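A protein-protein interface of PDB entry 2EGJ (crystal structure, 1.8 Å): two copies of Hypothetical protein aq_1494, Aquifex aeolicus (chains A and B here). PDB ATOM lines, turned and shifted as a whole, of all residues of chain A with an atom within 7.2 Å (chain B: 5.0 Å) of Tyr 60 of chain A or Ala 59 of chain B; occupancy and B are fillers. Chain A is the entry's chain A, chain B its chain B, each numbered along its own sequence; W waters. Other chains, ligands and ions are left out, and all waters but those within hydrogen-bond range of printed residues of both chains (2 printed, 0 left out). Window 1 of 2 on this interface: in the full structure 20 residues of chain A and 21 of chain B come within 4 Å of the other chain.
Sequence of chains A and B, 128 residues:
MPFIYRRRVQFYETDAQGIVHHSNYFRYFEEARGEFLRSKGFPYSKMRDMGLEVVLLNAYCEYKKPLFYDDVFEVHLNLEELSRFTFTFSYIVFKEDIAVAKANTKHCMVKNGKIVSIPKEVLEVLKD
The backbone NH of Ala 59 of chain A lies within hydrogen-bond range of the backbone carbonyl oxygen of Cys 61 of chain B (2.9 Å).
The backbone carbonyl oxygen (O) of Cys 61 of chain A is in hydrogen-bond range of the backbone NH (N) of Ala 59 of chain B.
The backbone NH (N) of Tyr 63 of chain A lies within hydrogen-bond range of the backbone carbonyl oxygen (O) of Leu 57 of chain B.
The backbone NH of Tyr 60 of chain B lies within hydrogen-bond range of the backbone carbonyl oxygen of Asn 104 of chain B, at 2.9 Å.
The side-chain hydroxyl (OH) of Tyr 63 of chain A lies within hydrogen-bond range of the backbone carbonyl oxygen (O) of His 22 of chain A.
The backbone carbonyl oxygen (O) of Asn 58 of chain A is in hydrogen-bond range of the backbone NH (N) of Lys 106 of chain A, at 3.1 Å.
The backbone carbonyl oxygen of Lys 102 of chain A lies within hydrogen-bond range of the backbone NH of Glu 62 of chain A.
The side-chain sulfur (SG) of Cys 61 of chain A lies close to the side-chain hydroxyl (OH) of Tyr 63 of chain A, at 3.8 Å.
OE1 of Glu 62 of chain A lies within hydrogen-bond range of OH of Tyr 60 of chain A, at 2.7 Å.
Among the printed residues, merely in contact across the chains: His 22 of chain A with Phe 26 of chain B, His 22 of chain A with Leu 56 of chain B, Phe 26 of chain A with Phe 26 of chain B, Asn 58 of chain A with Tyr 60 of chain B, Asn 58 of chain A with Cys 61 of chain B, Ala 59 of chain A with Tyr 60 of chain B, Tyr 60 of chain A with Asn 58 of chain B, Tyr 60 of chain A with Ala 59 of chain B, Tyr 60 of chain A with Tyr 60 of chain B, Cys 61 of chain A with Asn 58 of chain B, Glu 62 of chain A with Leu 57 of chain B, Glu 62 of chain A with Asn 58 of chain B and Tyr 63 of chain A with Leu 56 of chain B.
Of the printed residues of chain B, Asn 58 of chain A touches Tyr 60 and Cys 61.
Printed residues of chain B within 4 Å of Ala 59 of chain A: Tyr 60 (3.3 Å) and Cys 61 (2.9 Å).
Tyr 60 of chain A touches just these residues of chain B: Asn 58, Ala 59 and Tyr 60.
Printed residues of chain B within 4 Å of Tyr 63 of chain A: Leu 56 (3.5 Å) and Leu 57 (2.8 Å).
Lys 102 of chain A touches none of the printed residues of chain B.
Printed residues of chain A within 4 Å of Phe 26 of chain B: His 22 (3.7 Å) and Phe 26 (3.4 Å).
Of the printed residues of chain A, Ala 59 of chain B touches Tyr 60 (3.3 Å) and Cys 61 (2.9 Å).
Asn 104 of chain B touches none of the printed residues of chain A.
Of the 9 printed residues of chain B, 7 touch a printed residue of chain A.
Printed residues of chain B that touch a printed residue of chain A: Phe 26, Leu 56, Leu 57, Asn 58, Ala 59, Tyr 60 and Cys 61.
Hydrophobic or aromatic side chains of chain B within 4 Å of the printed part of chain A: Phe 26, Leu 56 and Tyr 60.
Among the printed residues, 16 pairs touch across the chains.
Among the printed residues, no Asp or Glu carboxylate lies within 4 Å of a Lys or Arg side-chain nitrogen of the other chain.
Phe 26 of chain A touches its own counterpart, Phe 26 of chain B.
Asn 58 of chain A touches Tyr 60 of chain B, and with the chains exchanged Tyr 60 of chain A touches Asn 58 of chain B.
Asn 58 of chain A touches Cys 61 of chain B, and with the chains exchanged Cys 61 of chain A touches Asn 58 of chain B.
Ala 59 of chain A touches Tyr 60 of chain B, and with the chains exchanged Tyr 60 of chain A touches Ala 59 of chain B.
Of the 16 pairs that touch across the chains among the printed residues, 10 have their exchanged pair printed and touching as well.
Water W2 lies within hydrogen-bond range of NE2 of His 22 of chain A (2.7 Å) and O of Phe 26 of chain B (2.7 Å).
Water W1 bridges the backbone carbonyl oxygen (O) of Tyr 63 of chain A (2.9 Å) and the backbone carbonyl oxygen (O) of Leu 57 of chain B (3.3 Å).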
ATOM      1  N   HIS A  22      33.820  -4.108  -2.018  1.00  0.00           N
ATOM      2  CA  HIS A  22      32.613  -4.092  -2.864  1.00  0.00           C
ATOM      3  C   HIS A  22      32.872  -4.501  -4.313  1.00  0.00           C
ATOM      4  O   HIS A  22      32.001  -5.112  -4.963  1.00  0.00           O
ATOM      5  CB  HIS A  22      31.905  -2.723  -2.816  1.00  0.00           C
ATOM      6  CG  HIS A  22      32.660  -1.592  -3.441  1.00  0.00           C
ATOM      7  ND1 HIS A  22      33.645  -0.890  -2.777  1.00  0.00           N
ATOM      8  CD2 HIS A  22      32.519  -0.990  -4.648  1.00  0.00           C
ATOM      9  CE1 HIS A  22      34.113   0.061  -3.567  1.00  0.00           C
ATOM     10  NE2 HIS A  22      33.424   0.043  -4.693  1.00  0.00           N
ATOM     11  N   PHE A  26      31.310  -8.173  -7.865  1.00  0.00           N
ATOM     12  CA  PHE A  26      31.173  -8.356  -9.327  1.00  0.00           C
ATOM     13  C   PHE A  26      31.933  -9.575  -9.852  1.00  0.00           C
ATOM     14  O   PHE A  26      31.495 -10.228 -10.810  1.00  0.00           O
ATOM     15  CB  PHE A  26      31.547  -7.063 -10.056  1.00  0.00           C
ATOM     16  CG  PHE A  26      30.665  -5.914  -9.644  1.00  0.00           C
ATOM     17  CD1 PHE A  26      29.355  -5.824 -10.148  1.00  0.00           C
ATOM     18  CD2 PHE A  26      31.085  -5.009  -8.663  1.00  0.00           C
ATOM     19  CE1 PHE A  26      28.489  -4.789  -9.716  1.00  0.00           C
ATOM     20  CE2 PHE A  26      30.227  -3.980  -8.227  1.00  0.00           C
ATOM     21  CZ  PHE A  26      28.931  -3.872  -8.775  1.00  0.00           C
ATOM     22  N   PHE A  29      29.852 -12.562  -9.054  1.00  0.00           N
ATOM     23  CA  PHE A  29      28.737 -12.690 -10.003  1.00  0.00           C
ATOM     24  C   PHE A  29      29.215 -13.297 -11.326  1.00  0.00           C
ATOM     25  O   PHE A  29      28.519 -14.120 -11.947  1.00  0.00           O
ATOM     26  CB  PHE A  29      28.052 -11.343 -10.262  1.00  0.00           C
ATOM     27  CG  PHE A  29      27.561 -10.653  -8.991  1.00  0.00           C
ATOM     28  CD1 PHE A  29      27.110 -11.410  -7.903  1.00  0.00           C
ATOM     29  CD2 PHE A  29      27.561  -9.260  -8.897  1.00  0.00           C
ATOM     30  CE1 PHE A  29      26.650 -10.755  -6.720  1.00  0.00           C
ATOM     31  CE2 PHE A  29      27.134  -8.601  -7.735  1.00  0.00           C
ATOM     32  CZ  PHE A  29      26.674  -9.346  -6.650  1.00  0.00           C
ATOM     33  N   ASN A  58      25.825  -2.848 -18.234  1.00  0.00           N
ATOM     34  CA  ASN A  58      25.745  -2.176 -16.934  1.00  0.00           C
ATOM     35  C   ASN A  58      25.759  -3.169 -15.768  1.00  0.00           C
ATOM     36  O   ASN A  58      25.533  -4.388 -15.943  1.00  0.00           O
ATOM     37  CB  ASN A  58      24.580  -1.172 -16.877  1.00  0.00           C
ATOM     38  CG  ASN A  58      23.229  -1.835 -16.939  1.00  0.00           C
ATOM     39  OD1 ASN A  58      22.865  -2.623 -16.060  1.00  0.00           O
ATOM     40  ND2 ASN A  58      22.465  -1.518 -17.984  1.00  0.00           N
ATOM     41  N   ALA A  59      26.028  -2.666 -14.570  1.00  0.00           N
ATOM     42  CA  ALA A  59      26.089  -3.541 -13.406  1.00  0.00           C
ATOM     43  C   ALA A  59      25.670  -2.718 -12.199  1.00  0.00           C
ATOM     44  O   ALA A  59      26.007  -1.535 -12.107  1.00  0.00           O
ATOM     45  CB  ALA A  59      27.505  -4.095 -13.226  1.00  0.00           C
ATOM     46  N   TYR A  60      24.901  -3.339 -11.304  1.00  0.00           N
ATOM     47  CA  TYR A  60      24.405  -2.662 -10.109  1.00  0.00           C
ATOM     48  C   TYR A  60      24.536  -3.629  -8.956  1.00  0.00           C
ATOM     49  O   TYR A  60      24.265  -4.818  -9.129  1.00  0.00           O
ATOM     50  CB  TYR A  60      22.924  -2.336 -10.287  1.00  0.00           C
ATOM     51  CG  TYR A  60      22.266  -1.858  -9.006  1.00  0.00           C
ATOM     52  CD1 TYR A  60      22.410  -0.541  -8.596  1.00  0.00           C
ATOM     53  CD2 TYR A  60      21.486  -2.731  -8.225  1.00  0.00           C
ATOM     54  CE1 TYR A  60      21.816  -0.082  -7.405  1.00  0.00           C
ATOM     55  CE2 TYR A  60      20.874  -2.279  -7.028  1.00  0.00           C
ATOM     56  CZ  TYR A  60      21.042  -0.952  -6.644  1.00  0.00           C
ATOM     57  OH  TYR A  60      20.447  -0.484  -5.481  1.00  0.00           O
ATOM     58  N   CYS A  61      24.963  -3.144  -7.789  1.00  0.00           N
ATOM     59  CA  CYS A  61      24.939  -3.976  -6.586  1.00  0.00           C
ATOM     60  C   CYS A  61      24.517  -3.106  -5.418  1.00  0.00           C
ATOM     61  O   CYS A  61      24.948  -1.956  -5.299  1.00  0.00           O
ATOM     62  CB  CYS A  61      26.316  -4.597  -6.274  1.00  0.00           C
ATOM     63  SG  CYS A  61      26.217  -5.942  -5.049  1.00  0.00           S
ATOM     64  N   GLU A  62      23.675  -3.672  -4.567  1.00  0.00           N
ATOM     65  CA  GLU A  62      23.359  -3.022  -3.289  1.00  0.00           C
ATOM     66  C   GLU A  62      23.806  -3.925  -2.145  1.00  0.00           C
ATOM     67  O   GLU A  62      23.645  -5.144  -2.207  1.00  0.00           O
ATOM     68  CB  GLU A  62      21.893  -2.676  -3.200  1.00  0.00           C
ATOM     69  CG  GLU A  62      20.947  -3.772  -3.552  1.00  0.00           C
ATOM     70  CD  GLU A  62      19.507  -3.310  -3.423  1.00  0.00           C
ATOM     71  OE1 GLU A  62      19.143  -2.210  -3.933  1.00  0.00           O
ATOM     72  OE2 GLU A  62      18.749  -4.059  -2.785  1.00  0.00           O
ATOM     73  N   TYR A  63      24.407  -3.325  -1.128  1.00  0.00           N
ATOM     74  CA  TYR A  63      25.116  -4.081  -0.102  1.00  0.00           C
ATOM     75  C   TYR A  63      24.343  -3.934   1.190  1.00  0.00           C
ATOM     76  O   TYR A  63      24.097  -2.812   1.632  1.00  0.00           O
ATOM     77  CB  TYR A  63      26.546  -3.533   0.053  1.00  0.00           C
ATOM     78  CG  TYR A  63      27.307  -3.587  -1.257  1.00  0.00           C
ATOM     79  CD1 TYR A  63      28.095  -4.697  -1.571  1.00  0.00           C
ATOM     80  CD2 TYR A  63      27.213  -2.548  -2.192  1.00  0.00           C
ATOM     81  CE1 TYR A  63      28.791  -4.763  -2.781  1.00  0.00           C
ATOM     82  CE2 TYR A  63      27.877  -2.621  -3.429  1.00  0.00           C
ATOM     83  CZ  TYR A  63      28.670  -3.737  -3.706  1.00  0.00           C
ATOM     84  OH  TYR A  63      29.343  -3.807  -4.909  1.00  0.00           O
ATOM     85  N   PHE A  89      20.779 -10.610 -15.876  1.00  0.00           N
ATOM     86  CA  PHE A  89      20.733 -11.532 -14.759  1.00  0.00           C
ATOM     87  C   PHE A  89      20.530 -10.731 -13.495  1.00  0.00           C
ATOM     88  O   PHE A  89      21.090  -9.636 -13.371  1.00  0.00           O
ATOM     89  CB  PHE A  89      22.089 -12.222 -14.613  1.00  0.00           C
ATOM     90  CG  PHE A  89      22.324 -13.287 -15.604  1.00  0.00           C
ATOM     91  CD1 PHE A  89      21.555 -14.439 -15.573  1.00  0.00           C
ATOM     92  CD2 PHE A  89      23.314 -13.154 -16.581  1.00  0.00           C
ATOM     93  CE1 PHE A  89      21.760 -15.450 -16.518  1.00  0.00           C
ATOM     94  CE2 PHE A  89      23.529 -14.175 -17.522  1.00  0.00           C
ATOM     95  CZ  PHE A  89      22.735 -15.314 -17.481  1.00  0.00           C
ATOM     96  N   TYR A  91      21.014 -11.258  -9.186  1.00  0.00           N
ATOM     97  CA  TYR A  91      21.744 -12.062  -8.208  1.00  0.00           C
ATOM     98  C   TYR A  91      21.230 -11.668  -6.839  1.00  0.00           C
ATOM     99  O   TYR A  91      20.979 -10.493  -6.591  1.00  0.00           O
ATOM    100  CB  TYR A  91      23.241 -11.736  -8.258  1.00  0.00           C
ATOM    101  CG  TYR A  91      23.791 -11.654  -9.675  1.00  0.00           C
ATOM    102  CD1 TYR A  91      24.433 -12.742 -10.243  1.00  0.00           C
ATOM    103  CD2 TYR A  91      23.677 -10.467 -10.430  1.00  0.00           C
ATOM    104  CE1 TYR A  91      24.946 -12.686 -11.552  1.00  0.00           C
ATOM    105  CE2 TYR A  91      24.186 -10.401 -11.761  1.00  0.00           C
ATOM    106  CZ  TYR A  91      24.822 -11.525 -12.292  1.00  0.00           C
ATOM    107  OH  TYR A  91      25.357 -11.471 -13.561  1.00  0.00           O
ATOM    108  N   LYS A 102      22.157  -7.616  -3.224  1.00  0.00           N
ATOM    109  CA  LYS A 102      21.290  -7.867  -4.379  1.00  0.00           C
ATOM    110  C   LYS A 102      21.886  -7.118  -5.559  1.00  0.00           C
ATOM    111  O   LYS A 102      22.336  -5.992  -5.414  1.00  0.00           O
ATOM    112  CB  LYS A 102      19.865  -7.370  -4.121  1.00  0.00           C
ATOM    113  CG  LYS A 102      19.079  -8.246  -3.158  1.00  0.00           C
ATOM    114  CD  LYS A 102      17.600  -7.735  -2.990  1.00  0.00           C
ATOM    115  CE  LYS A 102      16.756  -8.771  -2.223  1.00  0.00           C
ATOM    116  NZ  LYS A 102      15.564  -8.180  -1.497  1.00  0.00           N
ATOM    117  N   ALA A 103      21.859  -7.739  -6.736  1.00  0.00           N
ATOM    118  CA  ALA A 103      22.546  -7.155  -7.875  1.00  0.00           C
ATOM    119  C   ALA A 103      21.884  -7.519  -9.190  1.00  0.00           C
ATOM    120  O   ALA A 103      21.005  -8.395  -9.253  1.00  0.00           O
ATOM    121  CB  ALA A 103      24.001  -7.629  -7.879  1.00  0.00           C
ATOM    122  N   ASN A 104      22.318  -6.830 -10.243  1.00  0.00           N
ATOM    123  CA  ASN A 104      21.962  -7.240 -11.600  1.00  0.00           C
ATOM    124  C   ASN A 104      23.012  -6.799 -12.609  1.00  0.00           C
ATOM    125  O   ASN A 104      23.760  -5.835 -12.381  1.00  0.00           O
ATOM    126  CB  ASN A 104      20.547  -6.779 -11.981  1.00  0.00           C
ATOM    127  CG  ASN A 104      20.338  -5.278 -11.830  1.00  0.00           C
ATOM    128  OD1 ASN A 104      20.889  -4.486 -12.588  1.00  0.00           O
ATOM    129  ND2 ASN A 104      19.495  -4.886 -10.869  1.00  0.00           N
ATOM    130  N   THR A 105      23.084  -7.520 -13.720  1.00  0.00           N
ATOM    131  CA  THR A 105      23.997  -7.133 -14.795  1.00  0.00           C
ATOM    132  C   THR A 105      23.251  -7.293 -16.116  1.00  0.00           C
ATOM    133  O   THR A 105      22.395  -8.176 -16.245  1.00  0.00           O
ATOM    134  CB  THR A 105      25.281  -8.014 -14.825  1.00  0.00           C
ATOM    135  OG1 THR A 105      24.918  -9.382 -14.927  1.00  0.00           O
ATOM    136  CG2 THR A 105      26.175  -7.825 -13.571  1.00  0.00           C
ATOM    137  N   LYS A 106      23.578  -6.445 -17.076  1.00  0.00           N
ATOM    138  CA  LYS A 106      22.964  -6.479 -18.423  1.00  0.00           C
ATOM    139  C   LYS A 106      24.060  -6.620 -19.449  1.00  0.00           C
ATOM    140  O   LYS A 106      25.123  -5.989 -19.334  1.00  0.00           O
ATOM    141  CB  LYS A 106      22.164  -5.214 -18.692  1.00  0.00           C
ATOM    142  CG  LYS A 106      21.568  -5.139 -20.101  1.00  0.00           C
ATOM    143  CD  LYS A 106      20.785  -3.837 -20.291  1.00  0.00           C
ATOM    144  CE  LYS A 106      19.961  -3.848 -21.581  1.00  0.00           C
ATOM    145  NZ  LYS A 106      19.082  -2.590 -21.633  1.00  0.00           N
ATOM    146  N   PHE B  26      35.141   0.241 -10.298  1.00  0.00           N
ATOM    147  CA  PHE B  26      34.783   0.611  -8.916  1.00  0.00           C
ATOM    148  C   PHE B  26      36.018   0.974  -8.077  1.00  0.00           C
ATOM    149  O   PHE B  26      35.952   1.859  -7.212  1.00  0.00           O
ATOM    150  CB  PHE B  26      33.942  -0.500  -8.289  1.00  0.00           C
ATOM    151  CG  PHE B  26      32.659  -0.729  -9.057  1.00  0.00           C
ATOM    152  CD1 PHE B  26      31.592   0.165  -8.921  1.00  0.00           C
ATOM    153  CD2 PHE B  26      32.560  -1.785  -9.951  1.00  0.00           C
ATOM    154  CE1 PHE B  26      30.406   0.001  -9.689  1.00  0.00           C
ATOM    155  CE2 PHE B  26      31.378  -1.964 -10.735  1.00  0.00           C
ATOM    156  CZ  PHE B  26      30.309  -1.094 -10.577  1.00  0.00           C
ATOM    157  N   LEU B  56      29.608   1.701   1.943  1.00  0.00           N
ATOM    158  CA  LEU B  56      28.982   1.796   0.621  1.00  0.00           C
ATOM    159  C   LEU B  56      27.627   1.104   0.666  1.00  0.00           C
ATOM    160  O   LEU B  56      27.532  -0.034   1.124  1.00  0.00           O
ATOM    161  CB  LEU B  56      29.852   1.098  -0.423  1.00  0.00           C
ATOM    162  CG  LEU B  56      29.215   1.073  -1.822  1.00  0.00           C
ATOM    163  CD1 LEU B  56      29.347   2.434  -2.445  1.00  0.00           C
ATOM    164  CD2 LEU B  56      29.908   0.063  -2.665  1.00  0.00           C
ATOM    165  N   LEU B  57      26.579   1.781   0.212  1.00  0.00           N
ATOM    166  CA  LEU B  57      25.251   1.192   0.224  1.00  0.00           C
ATOM    167  C   LEU B  57      24.905   0.555  -1.124  1.00  0.00           C
ATOM    168  O   LEU B  57      24.343  -0.538  -1.177  1.00  0.00           O
ATOM    169  CB  LEU B  57      24.215   2.243   0.586  1.00  0.00           C
ATOM    170  CG  LEU B  57      24.357   2.784   2.015  1.00  0.00           C
ATOM    171  CD1 LEU B  57      23.470   4.020   2.150  1.00  0.00           C
ATOM    172  CD2 LEU B  57      23.969   1.676   2.991  1.00  0.00           C
ATOM    173  N   ASN B  58      25.248   1.247  -2.196  1.00  0.00           N
ATOM    174  CA  ASN B  58      25.065   0.689  -3.550  1.00  0.00           C
ATOM    175  C   ASN B  58      26.004   1.345  -4.557  1.00  0.00           C
ATOM    176  O   ASN B  58      26.554   2.433  -4.316  1.00  0.00           O
ATOM    177  CB  ASN B  58      23.591   0.749  -4.006  1.00  0.00           C
ATOM    178  CG  ASN B  58      23.057   2.164  -4.128  1.00  0.00           C
ATOM    179  OD1 ASN B  58      23.497   2.958  -4.968  1.00  0.00           O
ATOM    180  ND2 ASN B  58      22.095   2.488  -3.286  1.00  0.00           N
ATOM    181  N   ALA B  59      26.176   0.673  -5.696  1.00  0.00           N
ATOM    182  CA  ALA B  59      27.063   1.138  -6.750  1.00  0.00           C
ATOM    183  C   ALA B  59      26.447   0.724  -8.086  1.00  0.00           C
ATOM    184  O   ALA B  59      25.800  -0.342  -8.208  1.00  0.00           O
ATOM    185  CB  ALA B  59      28.471   0.526  -6.609  1.00  0.00           C
ATOM    186  N   TYR B  60      26.627   1.583  -9.076  1.00  0.00           N
ATOM    187  CA  TYR B  60      26.062   1.330 -10.406  1.00  0.00           C
ATOM    188  C   TYR B  60      27.048   1.839 -11.427  1.00  0.00           C
ATOM    189  O   TYR B  60      27.645   2.898 -11.240  1.00  0.00           O
ATOM    190  CB  TYR B  60      24.736   2.062 -10.556  1.00  0.00           C
ATOM    191  CG  TYR B  60      24.200   1.993 -11.968  1.00  0.00           C
ATOM    192  CD1 TYR B  60      23.670   0.801 -12.461  1.00  0.00           C
ATOM    193  CD2 TYR B  60      24.248   3.109 -12.810  1.00  0.00           C
ATOM    194  CE1 TYR B  60      23.174   0.720 -13.785  1.00  0.00           C
ATOM    195  CE2 TYR B  60      23.758   3.039 -14.141  1.00  0.00           C
ATOM    196  CZ  TYR B  60      23.241   1.831 -14.612  1.00  0.00           C
ATOM    197  OH  TYR B  60      22.736   1.744 -15.911  1.00  0.00           O
ATOM    198  N   CYS B  61      27.257   1.084 -12.501  1.00  0.00           N
ATOM    199  CA  CYS B  61      28.129   1.588 -13.563  1.00  0.00           C
ATOM    200  C   CYS B  61      27.543   1.165 -14.899  1.00  0.00           C
ATOM    201  O   CYS B  61      27.111   0.013 -15.047  1.00  0.00           O
ATOM    202  CB  CYS B  61      29.560   1.055 -13.429  1.00  0.00           C
ATOM    203  SG  CYS B  61      30.740   1.890 -14.572  1.00  0.00           S
ATOM    204  N   ASN B 104      27.536   5.758 -10.377  1.00  0.00           N
ATOM    205  CA  ASN B 104      27.267   6.435  -9.113  1.00  0.00           C
ATOM    206  C   ASN B 104      27.440   5.471  -7.964  1.00  0.00           C
ATOM    207  O   ASN B 104      27.377   4.247  -8.147  1.00  0.00           O
ATOM    208  CB  ASN B 104      25.866   7.085  -9.125  1.00  0.00           C
ATOM    209  CG  ASN B 104      24.730   6.078  -9.312  1.00  0.00           C
ATOM    210  OD1 ASN B 104      24.431   5.285  -8.445  1.00  0.00           O
ATOM    211  ND2 ASN B 104      24.060   6.166 -10.448  1.00  0.00           N
ATOM    212  N   THR B 105      27.678   6.023  -6.768  1.00  0.00           N
ATOM    213  CA  THR B 105      27.777   5.228  -5.555  1.00  0.00           C
ATOM    214  C   THR B 105      27.084   6.007  -4.440  1.00  0.00           C
ATOM    215  O   THR B 105      27.155   7.237  -4.415  1.00  0.00           O
ATOM    216  CB  THR B 105      29.251   4.960  -5.125  1.00  0.00           C
ATOM    217  OG1 THR B 105      29.986   6.188  -4.969  1.00  0.00           O
ATOM    218  CG2 THR B 105      29.960   4.040  -6.139  1.00  0.00           C
HETATM  219  O   HOH W   1      21.842  -1.136   0.818  1.00  0.00           O
HETATM  220  O   HOH W   2      33.721   2.509  -5.791  1.00  0.00           O
